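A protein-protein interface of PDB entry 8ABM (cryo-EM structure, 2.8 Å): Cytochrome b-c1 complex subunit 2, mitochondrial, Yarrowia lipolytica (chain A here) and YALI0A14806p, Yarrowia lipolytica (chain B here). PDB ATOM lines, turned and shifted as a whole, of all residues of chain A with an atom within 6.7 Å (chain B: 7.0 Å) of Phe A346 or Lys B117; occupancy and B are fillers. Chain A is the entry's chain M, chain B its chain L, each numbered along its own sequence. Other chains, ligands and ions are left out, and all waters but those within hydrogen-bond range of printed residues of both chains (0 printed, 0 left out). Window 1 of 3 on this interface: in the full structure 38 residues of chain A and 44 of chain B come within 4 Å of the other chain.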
ATOM      1  N   TYR A 341       7.295   3.103 -27.444  1.00  0.00           N
ATOM      2  CA  TYR A 341       7.176   1.926 -28.280  1.00  0.00           C
ATOM      3  C   TYR A 341       5.930   1.143 -27.892  1.00  0.00           C
ATOM      4  O   TYR A 341       5.222   0.631 -28.753  1.00  0.00           O
ATOM      5  CB  TYR A 341       8.382   1.020 -28.050  1.00  0.00           C
ATOM      6  CG  TYR A 341       8.282  -0.334 -28.696  1.00  0.00           C
ATOM      7  CD1 TYR A 341       8.113  -0.460 -30.068  1.00  0.00           C
ATOM      8  CD2 TYR A 341       8.413  -1.491 -27.944  1.00  0.00           C
ATOM      9  CE1 TYR A 341       8.049  -1.703 -30.678  1.00  0.00           C
ATOM     10  CE2 TYR A 341       8.357  -2.742 -28.540  1.00  0.00           C
ATOM     11  CZ  TYR A 341       8.168  -2.849 -29.909  1.00  0.00           C
ATOM     12  OH  TYR A 341       8.110  -4.074 -30.510  1.00  0.00           O
ATOM     13  N   ALA A 342       5.703   1.046 -26.582  1.00  0.00           N
ATOM     14  CA  ALA A 342       4.596   0.265 -26.069  1.00  0.00           C
ATOM     15  C   ALA A 342       3.282   0.947 -26.413  1.00  0.00           C
ATOM     16  O   ALA A 342       2.378   0.295 -26.923  1.00  0.00           O
ATOM     17  CB  ALA A 342       4.741   0.046 -24.590  1.00  0.00           C
ATOM     18  N   LYS A 343       3.203   2.255 -26.153  1.00  0.00           N
ATOM     19  CA  LYS A 343       1.978   2.989 -26.419  1.00  0.00           C
ATOM     20  C   LYS A 343       1.701   2.986 -27.920  1.00  0.00           C
ATOM     21  O   LYS A 343       0.544   3.046 -28.328  1.00  0.00           O
ATOM     22  CB  LYS A 343       2.046   4.425 -25.884  1.00  0.00           C
ATOM     23  CG  LYS A 343       1.918   4.593 -24.372  1.00  0.00           C
ATOM     24  CD  LYS A 343       0.698   5.394 -23.924  1.00  0.00           C
ATOM     25  CE  LYS A 343       1.015   6.814 -23.501  1.00  0.00           C
ATOM     26  NZ  LYS A 343      -0.069   7.762 -23.866  1.00  0.00           N
ATOM     27  N   SER A 344       2.764   2.930 -28.733  1.00  0.00           N
ATOM     28  CA  SER A 344       2.566   3.055 -30.166  1.00  0.00           C
ATOM     29  C   SER A 344       2.148   1.728 -30.793  1.00  0.00           C
ATOM     30  O   SER A 344       1.316   1.738 -31.694  1.00  0.00           O
ATOM     31  CB  SER A 344       3.739   3.684 -30.869  1.00  0.00           C
ATOM     32  OG  SER A 344       4.879   2.848 -30.791  1.00  0.00           O
ATOM     33  N   LYS A 345       2.752   0.614 -30.344  1.00  0.00           N
ATOM     34  CA  LYS A 345       2.349  -0.714 -30.785  1.00  0.00           C
ATOM     35  C   LYS A 345       0.871  -0.911 -30.495  1.00  0.00           C
ATOM     36  O   LYS A 345       0.141  -1.465 -31.312  1.00  0.00           O
ATOM     37  CB  LYS A 345       3.026  -1.814 -29.967  1.00  0.00           C
ATOM     38  CG  LYS A 345       3.989  -2.690 -30.742  1.00  0.00           C
ATOM     39  CD  LYS A 345       4.039  -4.112 -30.225  1.00  0.00           C
ATOM     40  CE  LYS A 345       4.974  -4.284 -29.045  1.00  0.00           C
ATOM     41  NZ  LYS A 345       5.482  -5.673 -28.942  1.00  0.00           N
ATOM     42  N   PHE A 346       0.456  -0.465 -29.307  1.00  0.00           N
ATOM     43  CA  PHE A 346      -0.911  -0.663 -28.883  1.00  0.00           C
ATOM     44  C   PHE A 346      -1.833   0.162 -29.763  1.00  0.00           C
ATOM     45  O   PHE A 346      -2.882  -0.323 -30.158  1.00  0.00           O
ATOM     46  CB  PHE A 346      -1.125  -0.247 -27.432  1.00  0.00           C
ATOM     47  CG  PHE A 346      -2.551  -0.434 -26.981  1.00  0.00           C
ATOM     48  CD1 PHE A 346      -3.053  -1.704 -26.718  1.00  0.00           C
ATOM     49  CD2 PHE A 346      -3.394   0.657 -26.820  1.00  0.00           C
ATOM     50  CE1 PHE A 346      -4.368  -1.878 -26.310  1.00  0.00           C
ATOM     51  CE2 PHE A 346      -4.706   0.482 -26.401  1.00  0.00           C
ATOM     52  CZ  PHE A 346      -5.194  -0.783 -26.158  1.00  0.00           C
ATOM     53  N   ALA A 347      -1.445   1.410 -30.035  1.00  0.00           N
ATOM     54  CA  ALA A 347      -2.303   2.255 -30.843  1.00  0.00           C
ATOM     55  C   ALA A 347      -2.507   1.607 -32.209  1.00  0.00           C
ATOM     56  O   ALA A 347      -3.621   1.613 -32.732  1.00  0.00           O
ATOM     57  CB  ALA A 347      -1.739   3.645 -30.947  1.00  0.00           C
ATOM     58  N   ALA A 348      -1.437   1.006 -32.747  1.00  0.00           N
ATOM     59  CA  ALA A 348      -1.505   0.397 -34.065  1.00  0.00           C
ATOM     60  C   ALA A 348      -2.447  -0.802 -34.050  1.00  0.00           C
ATOM     61  O   ALA A 348      -3.217  -0.986 -34.989  1.00  0.00           O
ATOM     62  CB  ALA A 348      -0.135   0.015 -34.554  1.00  0.00           C
ATOM     63  N   ALA A 349      -2.397  -1.582 -32.963  1.00  0.00           N
ATOM     64  CA  ALA A 349      -3.178  -2.804 -32.851  1.00  0.00           C
ATOM     65  C   ALA A 349      -4.668  -2.478 -32.798  1.00  0.00           C
ATOM     66  O   ALA A 349      -5.427  -3.040 -33.573  1.00  0.00           O
ATOM     67  CB  ALA A 349      -2.730  -3.608 -31.660  1.00  0.00           C
ATOM     68  N   GLU A 350      -5.062  -1.540 -31.930  1.00  0.00           N
ATOM     69  CA  GLU A 350      -6.465  -1.197 -31.728  1.00  0.00           C
ATOM     70  C   GLU A 350      -7.059  -0.519 -32.965  1.00  0.00           C
ATOM     71  O   GLU A 350      -8.273  -0.604 -33.193  1.00  0.00           O
ATOM     72  CB  GLU A 350      -6.648  -0.395 -30.440  1.00  0.00           C
ATOM     73  CG  GLU A 350      -6.082   1.007 -30.538  1.00  0.00           C
ATOM     74  CD  GLU A 350      -6.078   1.860 -29.287  1.00  0.00           C
ATOM     75  OE1 GLU A 350      -5.126   2.664 -29.140  1.00  0.00           O
ATOM     76  OE2 GLU A 350      -7.024   1.734 -28.481  1.00  0.00           O
ATOM     77  N   ALA A 351      -6.202   0.125 -33.774  1.00  0.00           N
ATOM     78  CA  ALA A 351      -6.631   0.738 -35.021  1.00  0.00           C
ATOM     79  C   ALA A 351      -7.015  -0.343 -36.029  1.00  0.00           C
ATOM     80  O   ALA A 351      -8.006  -0.226 -36.742  1.00  0.00           O
ATOM     81  CB  ALA A 351      -5.552   1.643 -35.565  1.00  0.00           C
ATOM     82  N   GLU A 353      -8.059  -3.161 -35.300  1.00  0.00           N
ATOM     83  CA  GLU A 353      -9.165  -3.935 -34.752  1.00  0.00           C
ATOM     84  C   GLU A 353     -10.497  -3.246 -35.023  1.00  0.00           C
ATOM     85  O   GLU A 353     -11.405  -3.895 -35.542  1.00  0.00           O
ATOM     86  CB  GLU A 353      -8.977  -4.239 -33.267  1.00  0.00           C
ATOM     87  CG  GLU A 353      -8.025  -5.403 -33.013  1.00  0.00           C
ATOM     88  CD  GLU A 353      -7.012  -5.180 -31.896  1.00  0.00           C
ATOM     89  OE1 GLU A 353      -7.344  -4.432 -30.952  1.00  0.00           O
ATOM     90  OE2 GLU A 353      -5.855  -5.675 -32.010  1.00  0.00           O
ATOM     91  N   PRO A 375       0.966  -4.238 -36.506  1.00  0.00           N
ATOM     92  CA  PRO A 375       1.309  -3.868 -35.129  1.00  0.00           C
ATOM     93  C   PRO A 375       2.519  -4.589 -34.530  1.00  0.00           C
ATOM     94  O   PRO A 375       3.243  -4.012 -33.719  1.00  0.00           O
ATOM     95  CB  PRO A 375       0.016  -4.125 -34.336  1.00  0.00           C
ATOM     96  CG  PRO A 375      -0.820  -4.996 -35.247  1.00  0.00           C
ATOM     97  CD  PRO A 375      -0.464  -4.547 -36.648  1.00  0.00           C
ATOM     98  N   VAL A 378       5.851  -2.673 -35.812  1.00  0.00           N
ATOM     99  CA  VAL A 378       6.033  -1.294 -35.404  1.00  0.00           C
ATOM    100  C   VAL A 378       7.445  -1.143 -34.851  1.00  0.00           C
ATOM    101  O   VAL A 378       7.866  -1.897 -33.975  1.00  0.00           O
ATOM    102  CB  VAL A 378       4.937  -0.892 -34.398  1.00  0.00           C
ATOM    103  CG1 VAL A 378       5.277   0.349 -33.586  1.00  0.00           C
ATOM    104  CG2 VAL A 378       3.603  -0.720 -35.100  1.00  0.00           C
ATOM    105  N   GLN B  50      -4.817  -9.005 -31.798  1.00  0.00           N
ATOM    106  CA  GLN B  50      -3.488  -8.883 -31.224  1.00  0.00           C
ATOM    107  C   GLN B  50      -3.564  -8.237 -29.844  1.00  0.00           C
ATOM    108  O   GLN B  50      -2.569  -8.177 -29.130  1.00  0.00           O
ATOM    109  CB  GLN B  50      -2.571  -8.148 -32.207  1.00  0.00           C
ATOM    110  CG  GLN B  50      -1.759  -9.104 -33.072  1.00  0.00           C
ATOM    111  CD  GLN B  50      -0.265  -9.005 -32.868  1.00  0.00           C
ATOM    112  OE1 GLN B  50       0.371  -8.043 -33.293  1.00  0.00           O
ATOM    113  NE2 GLN B  50       0.319 -10.014 -32.237  1.00  0.00           N
ATOM    114  N   THR B  51      -4.766  -7.789 -29.484  1.00  0.00           N
ATOM    115  CA  THR B  51      -5.027  -7.113 -28.232  1.00  0.00           C
ATOM    116  C   THR B  51      -5.921  -7.995 -27.368  1.00  0.00           C
ATOM    117  O   THR B  51      -6.706  -8.777 -27.891  1.00  0.00           O
ATOM    118  CB  THR B  51      -5.591  -5.735 -28.584  1.00  0.00           C
ATOM    119  OG1 THR B  51      -4.476  -4.848 -28.492  1.00  0.00           O
ATOM    120  CG2 THR B  51      -6.815  -5.311 -27.803  1.00  0.00           C
ATOM    121  N   ALA B  52      -5.842  -7.822 -26.044  1.00  0.00           N
ATOM    122  CA  ALA B  52      -6.709  -8.545 -25.125  1.00  0.00           C
ATOM    123  C   ALA B  52      -7.427  -7.588 -24.176  1.00  0.00           C
ATOM    124  O   ALA B  52      -6.895  -6.538 -23.841  1.00  0.00           O
ATOM    125  CB  ALA B  52      -5.884  -9.545 -24.370  1.00  0.00           C
ATOM    126  N   THR B  53      -8.648  -7.941 -23.762  1.00  0.00           N
ATOM    127  CA  THR B  53      -9.299  -7.259 -22.657  1.00  0.00           C
ATOM    128  C   THR B  53      -9.438  -8.250 -21.507  1.00  0.00           C
ATOM    129  O   THR B  53     -10.236  -9.169 -21.608  1.00  0.00           O
ATOM    130  CB  THR B  53     -10.662  -6.683 -23.077  1.00  0.00           C
ATOM    131  OG1 THR B  53     -10.431  -5.757 -24.138  1.00  0.00           O
ATOM    132  CG2 THR B  53     -11.368  -5.964 -21.951  1.00  0.00           C
ATOM    133  N   VAL B  54      -8.658  -8.092 -20.434  1.00  0.00           N
ATOM    134  CA  VAL B  54      -8.964  -8.791 -19.196  1.00  0.00           C
ATOM    135  C   VAL B  54      -9.620  -7.817 -18.231  1.00  0.00           C
ATOM    136  O   VAL B  54      -9.326  -6.621 -18.235  1.00  0.00           O
ATOM    137  CB  VAL B  54      -7.740  -9.460 -18.553  1.00  0.00           C
ATOM    138  CG1 VAL B  54      -7.108 -10.444 -19.511  1.00  0.00           C
ATOM    139  CG2 VAL B  54      -6.724  -8.444 -18.054  1.00  0.00           C
ATOM    140  N   MET B  99       2.820  -0.402 -19.705  1.00  0.00           N
ATOM    141  CA  MET B  99       2.108  -1.525 -20.301  1.00  0.00           C
ATOM    142  C   MET B  99       1.849  -1.202 -21.767  1.00  0.00           C
ATOM    143  O   MET B  99       2.090  -2.024 -22.651  1.00  0.00           O
ATOM    144  CB  MET B  99       0.701  -1.640 -19.716  1.00  0.00           C
ATOM    145  CG  MET B  99       0.411  -2.715 -18.721  1.00  0.00           C
ATOM    146  SD  MET B  99      -1.347  -3.218 -18.964  1.00  0.00           S
ATOM    147  CE  MET B  99      -2.196  -1.680 -19.353  1.00  0.00           C
ATOM    148  N   GLY B 100       1.303  -0.002 -21.994  1.00  0.00           N
ATOM    149  CA  GLY B 100       0.918   0.368 -23.339  1.00  0.00           C
ATOM    150  C   GLY B 100      -0.578   0.620 -23.483  1.00  0.00           C
ATOM    151  O   GLY B 100      -0.976   1.546 -24.189  1.00  0.00           O
ATOM    152  N   GLY B 101      -1.397  -0.199 -22.814  1.00  0.00           N
ATOM    153  CA  GLY B 101      -2.837  -0.073 -22.950  1.00  0.00           C
ATOM    154  C   GLY B 101      -3.426   0.876 -21.912  1.00  0.00           C
ATOM    155  O   GLY B 101      -2.763   1.802 -21.460  1.00  0.00           O
ATOM    156  N   HIS B 102      -4.688   0.646 -21.550  1.00  0.00           N
ATOM    157  CA  HIS B 102      -5.344   1.477 -20.557  1.00  0.00           C
ATOM    158  C   HIS B 102      -6.183   0.614 -19.625  1.00  0.00           C
ATOM    159  O   HIS B 102      -6.451  -0.551 -19.917  1.00  0.00           O
ATOM    160  CB  HIS B 102      -6.174   2.580 -21.227  1.00  0.00           C
ATOM    161  CG  HIS B 102      -7.228   2.055 -22.137  1.00  0.00           C
ATOM    162  ND1 HIS B 102      -6.987   1.802 -23.468  1.00  0.00           N
ATOM    163  CD2 HIS B 102      -8.514   1.718 -21.909  1.00  0.00           C
ATOM    164  CE1 HIS B 102      -8.088   1.344 -24.030  1.00  0.00           C
ATOM    165  NE2 HIS B 102      -9.041   1.288 -23.094  1.00  0.00           N
ATOM    166  N   LEU B 103      -6.594   1.233 -18.510  1.00  0.00           N
ATOM    167  CA  LEU B 103      -7.537   0.675 -17.555  1.00  0.00           C
ATOM    168  C   LEU B 103      -8.822   1.476 -17.612  1.00  0.00           C
ATOM    169  O   LEU B 103      -8.815   2.639 -18.006  1.00  0.00           O
ATOM    170  CB  LEU B 103      -6.950   0.765 -16.147  1.00  0.00           C
ATOM    171  CG  LEU B 103      -6.271  -0.510 -15.673  1.00  0.00           C
ATOM    172  CD1 LEU B 103      -5.020  -0.808 -16.506  1.00  0.00           C
ATOM    173  CD2 LEU B 103      -5.909  -0.360 -14.210  1.00  0.00           C
ATOM    174  N   ASN B 104      -9.914   0.838 -17.205  1.00  0.00           N
ATOM    175  CA  ASN B 104     -11.190   1.516 -17.176  1.00  0.00           C
ATOM    176  C   ASN B 104     -12.057   0.848 -16.126  1.00  0.00           C
ATOM    177  O   ASN B 104     -11.873  -0.331 -15.838  1.00  0.00           O
ATOM    178  CB  ASN B 104     -11.881   1.490 -18.537  1.00  0.00           C
ATOM    179  CG  ASN B 104     -13.038   2.461 -18.580  1.00  0.00           C
ATOM    180  OD1 ASN B 104     -12.956   3.552 -18.019  1.00  0.00           O
ATOM    181  ND2 ASN B 104     -14.124   2.071 -19.226  1.00  0.00           N
ATOM    182  N   TYR B 115     -11.489  -3.139 -15.905  1.00  0.00           N
ATOM    183  CA  TYR B 115     -10.844  -3.922 -16.942  1.00  0.00           C
ATOM    184  C   TYR B 115      -9.631  -3.212 -17.512  1.00  0.00           C
ATOM    185  O   TYR B 115      -9.460  -2.007 -17.354  1.00  0.00           O
ATOM    186  CB  TYR B 115     -11.843  -4.299 -18.031  1.00  0.00           C
ATOM    187  CG  TYR B 115     -12.326  -3.161 -18.876  1.00  0.00           C
ATOM    188  CD1 TYR B 115     -11.622  -2.741 -19.994  1.00  0.00           C
ATOM    189  CD2 TYR B 115     -13.535  -2.553 -18.598  1.00  0.00           C
ATOM    190  CE1 TYR B 115     -12.102  -1.718 -20.798  1.00  0.00           C
ATOM    191  CE2 TYR B 115     -14.034  -1.537 -19.394  1.00  0.00           C
ATOM    192  CZ  TYR B 115     -13.314  -1.116 -20.500  1.00  0.00           C
ATOM    193  OH  TYR B 115     -13.801  -0.102 -21.274  1.00  0.00           O
ATOM    194  N   ALA B 116      -8.829  -3.992 -18.232  1.00  0.00           N
ATOM    195  CA  ALA B 116      -7.563  -3.528 -18.757  1.00  0.00           C
ATOM    196  C   ALA B 116      -7.405  -4.054 -20.174  1.00  0.00           C
ATOM    197  O   ALA B 116      -7.335  -5.267 -20.379  1.00  0.00           O
ATOM    198  CB  ALA B 116      -6.435  -4.000 -17.886  1.00  0.00           C
ATOM    199  N   LYS B 117      -7.372  -3.112 -21.120  1.00  0.00           N
ATOM    200  CA  LYS B 117      -7.115  -3.421 -22.510  1.00  0.00           C
ATOM    201  C   LYS B 117      -5.615  -3.316 -22.733  1.00  0.00           C
ATOM    202  O   LYS B 117      -5.010  -2.340 -22.312  1.00  0.00           O
ATOM    203  CB  LYS B 117      -7.901  -2.466 -23.404  1.00  0.00           C
ATOM    204  CG  LYS B 117      -8.188  -3.027 -24.781  1.00  0.00           C
ATOM    205  CD  LYS B 117      -9.168  -2.169 -25.560  1.00  0.00           C
ATOM    206  CE  LYS B 117      -9.224  -2.443 -27.049  1.00  0.00           C
ATOM    207  NZ  LYS B 117     -10.014  -3.653 -27.395  1.00  0.00           N
ATOM    208  N   SER B 118      -5.025  -4.347 -23.337  1.00  0.00           N
ATOM    209  CA  SER B 118      -3.580  -4.396 -23.459  1.00  0.00           C
ATOM    210  C   SER B 118      -3.175  -5.093 -24.750  1.00  0.00           C
ATOM    211  O   SER B 118      -3.999  -5.395 -25.608  1.00  0.00           O
ATOM    212  CB  SER B 118      -2.943  -5.061 -22.259  1.00  0.00           C
ATOM    213  OG  SER B 118      -3.365  -6.412 -22.144  1.00  0.00           O
ATOM    214  N   PHE B 119      -1.870  -5.317 -24.862  1.00  0.00           N
ATOM    215  CA  PHE B 119      -1.310  -6.138 -25.908  1.00  0.00           C
ATOM    216  C   PHE B 119      -1.323  -7.594 -25.453  1.00  0.00           C
ATOM    217  O   PHE B 119      -1.582  -7.862 -24.284  1.00  0.00           O
ATOM    218  CB  PHE B 119       0.058  -5.577 -26.287  1.00  0.00           C
ATOM    219  CG  PHE B 119       0.305  -5.752 -27.753  1.00  0.00           C
ATOM    220  CD1 PHE B 119      -0.352  -4.947 -28.670  1.00  0.00           C
ATOM    221  CD2 PHE B 119       1.084  -6.804 -28.215  1.00  0.00           C
ATOM    222  CE1 PHE B 119      -0.175  -5.156 -30.029  1.00  0.00           C
ATOM    223  CE2 PHE B 119       1.258  -7.011 -29.577  1.00  0.00           C
ATOM    224  CZ  PHE B 119       0.619  -6.189 -30.481  1.00  0.00           C
ATOM    225  N   ASP B 122       1.138  -8.548 -22.651  1.00  0.00           N
ATOM    226  CA  ASP B 122       1.048  -7.605 -21.548  1.00  0.00           C
ATOM    227  C   ASP B 122      -0.106  -7.983 -20.624  1.00  0.00           C
ATOM    228  O   ASP B 122      -0.537  -7.184 -19.792  1.00  0.00           O
ATOM    229  CB  ASP B 122       0.877  -6.178 -22.076  1.00  0.00           C
ATOM    230  CG  ASP B 122       2.177  -5.577 -22.586  1.00  0.00           C
ATOM    231  OD1 ASP B 122       3.223  -5.810 -21.939  1.00  0.00           O
ATOM    232  OD2 ASP B 122       2.139  -4.888 -23.628  1.00  0.00           O
ATOM    233  N   SER B 126      -1.256  -6.711 -16.552  1.00  0.00           N
ATOM    234  CA  SER B 126      -2.559  -6.109 -16.351  1.00  0.00           C
ATOM    235  C   SER B 126      -3.365  -6.890 -15.319  1.00  0.00           C
ATOM    236  O   SER B 126      -4.057  -6.279 -14.507  1.00  0.00           O
ATOM    237  CB  SER B 126      -3.293  -5.944 -17.648  1.00  0.00           C
ATOM    238  OG  SER B 126      -3.199  -7.118 -18.438  1.00  0.00           O
ATOM    239  N   GLY B 399     -15.560  -5.680 -31.008  1.00  0.00           N
ATOM    240  CA  GLY B 399     -14.195  -5.708 -30.500  1.00  0.00           C
ATOM    241  C   GLY B 399     -14.094  -6.493 -29.195  1.00  0.00           C
ATOM    242  O   GLY B 399     -15.098  -6.981 -28.677  1.00  0.00           O
ATOM    243  N   THR B 400     -12.869  -6.612 -28.674  1.00  0.00           N
ATOM    244  CA  THR B 400     -12.634  -7.487 -27.537  1.00  0.00           C
ATOM    245  C   THR B 400     -13.328  -6.954 -26.291  1.00  0.00           C
ATOM    246  O   THR B 400     -13.700  -7.739 -25.428  1.00  0.00           O
ATOM    247  CB  THR B 400     -11.145  -7.695 -27.250  1.00  0.00           C
ATOM    248  OG1 THR B 400     -10.610  -6.445 -26.824  1.00  0.00           O
ATOM    249  CG2 THR B 400     -10.378  -8.229 -28.437  1.00  0.00           C
ATOM    250  N   THR B 401     -13.482  -5.628 -26.201  1.00  0.00           N
ATOM    251  CA  THR B 401     -14.124  -5.039 -25.040  1.00  0.00           C
ATOM    252  C   THR B 401     -15.602  -5.412 -25.031  1.00  0.00           C
ATOM    253  O   THR B 401     -16.159  -5.642 -23.963  1.00  0.00           O
ATOM    254  CB  THR B 401     -13.863  -3.532 -24.932  1.00  0.00           C
ATOM    255  OG1 THR B 401     -12.447  -3.440 -24.822  1.00  0.00           O
ATOM    256  CG2 THR B 401     -14.453  -2.896 -23.690  1.00  0.00           C
ATOM    257  N   TYR B 402     -16.214  -5.474 -26.218  1.00  0.00           N
ATOM    258  CA  TYR B 402     -17.625  -5.803 -26.298  1.00  0.00           C
ATOM    259  C   TYR B 402     -17.848  -7.273 -25.987  1.00  0.00           C
ATOM    260  O   TYR B 402     -18.833  -7.628 -25.342  1.00  0.00           O
ATOM    261  CB  TYR B 402     -18.202  -5.446 -27.662  1.00  0.00           C
ATOM    262  CG  TYR B 402     -18.257  -3.965 -27.909  1.00  0.00           C
ATOM    263  CD1 TYR B 402     -19.056  -3.142 -27.127  1.00  0.00           C
ATOM    264  CD2 TYR B 402     -17.507  -3.386 -28.921  1.00  0.00           C
ATOM    265  CE1 TYR B 402     -19.110  -1.773 -27.348  1.00  0.00           C
ATOM    266  CE2 TYR B 402     -17.549  -2.019 -29.153  1.00  0.00           C
ATOM    267  CZ  TYR B 402     -18.353  -1.211 -28.364  1.00  0.00           C
ATOM    268  OH  TYR B 402     -18.403   0.135 -28.588  1.00  0.00           O
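The backbone NH (N) of Gln B50 is in hydrogen-bond range of the side-chain carboxylate (OE2) of Glu A353 (3.5 Å).
The side-chain carboxylate (OE2) of Glu A353 sits close to the backbone NH (N) of Thr B51 (3.5 Å).
Of the printed residues of chain B, Phe A346 touches Thr B51, Gly B100, Gly B101, His B102, Lys B117 and Ser B118.
Of the printed residues of chain A, Gln B50 touches Glu A353 and Pro A375.
Ala B52 touches none of the printed residues of chain A.
Of the printed residues of chain A, Met B99 touches Ala A342.
Of the printed residues of chain A, Lys B117 touches Phe A346 (3.99 Å).
Thr B401 touches none of the printed residues of chain A.
The nearest printed residue of chain B that does not touch Phe A346 is Phe B119 (4.2 Å).
The nearest printed residue of chain B that does not touch Lys A343 is Gly B101 (5.6 Å).
OG1 of Thr B51 sits at hydrogen-bond distance from O of Ser B118, at 3.0 Å.
OH of Tyr A341 is in hydrogen-bond range of NZ of Lys A345 (3.5 Å).
O of His B102 is in hydrogen-bond range of N of Lys B117, 3.0 Å away.
The side-chain hydroxyl (OG1) of Thr B400 lies within hydrogen-bond range of the side-chain amino group (NZ) of Lys B117 (2.9 Å).
The backbone carbonyl oxygen (O) of Ala B52 sits at hydrogen-bond distance from the backbone NH (N) of Ser B118 (2.9 Å).
Of the 22 printed residues of chain B, 9 touch a printed residue of chain A.
Printed residues of chain B that touch a printed residue of chain A: Gln B50, Thr B51, Met B99, Gly B100, Gly B101, His B102, Lys B117, Ser B118 and Phe B119.
Hydrophobic or aromatic side chains of chain B within 4 Å of the printed part of chain A: His B102 and Phe B119.
Along chain B the printed residues that touch a printed residue of chain A span positions 50 to 119.
Of the 14 printed residues of chain A, 7 touch a printed residue of chain B.
Printed residues of chain A that touch a printed residue of chain B: Ala A342, Lys A343, Lys A345, Phe A346, Ala A349, Glu A353 and Pro A375.
Hydrophobic or aromatic side chains of chain A within 4 Å of the printed part of chain B: Ala A342, Phe A346, Ala A349 and Pro A375.
Among the printed residues, merely in contact across the chains: Ala A342 with Met B99, Ala A342 with Gly B100, Lys A343 with Gly B100, Lys A345 with Phe B119, Phe A346 with Thr B51, Phe A346 with Gly B100, Phe A346 with Gly B101, Phe A346 with His B102, Phe A346 with Lys B117, Phe A346 with Ser B118, Ala A349 with Thr B51, Ala A349 with Phe B119 and Pro A375 with Gln B50.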
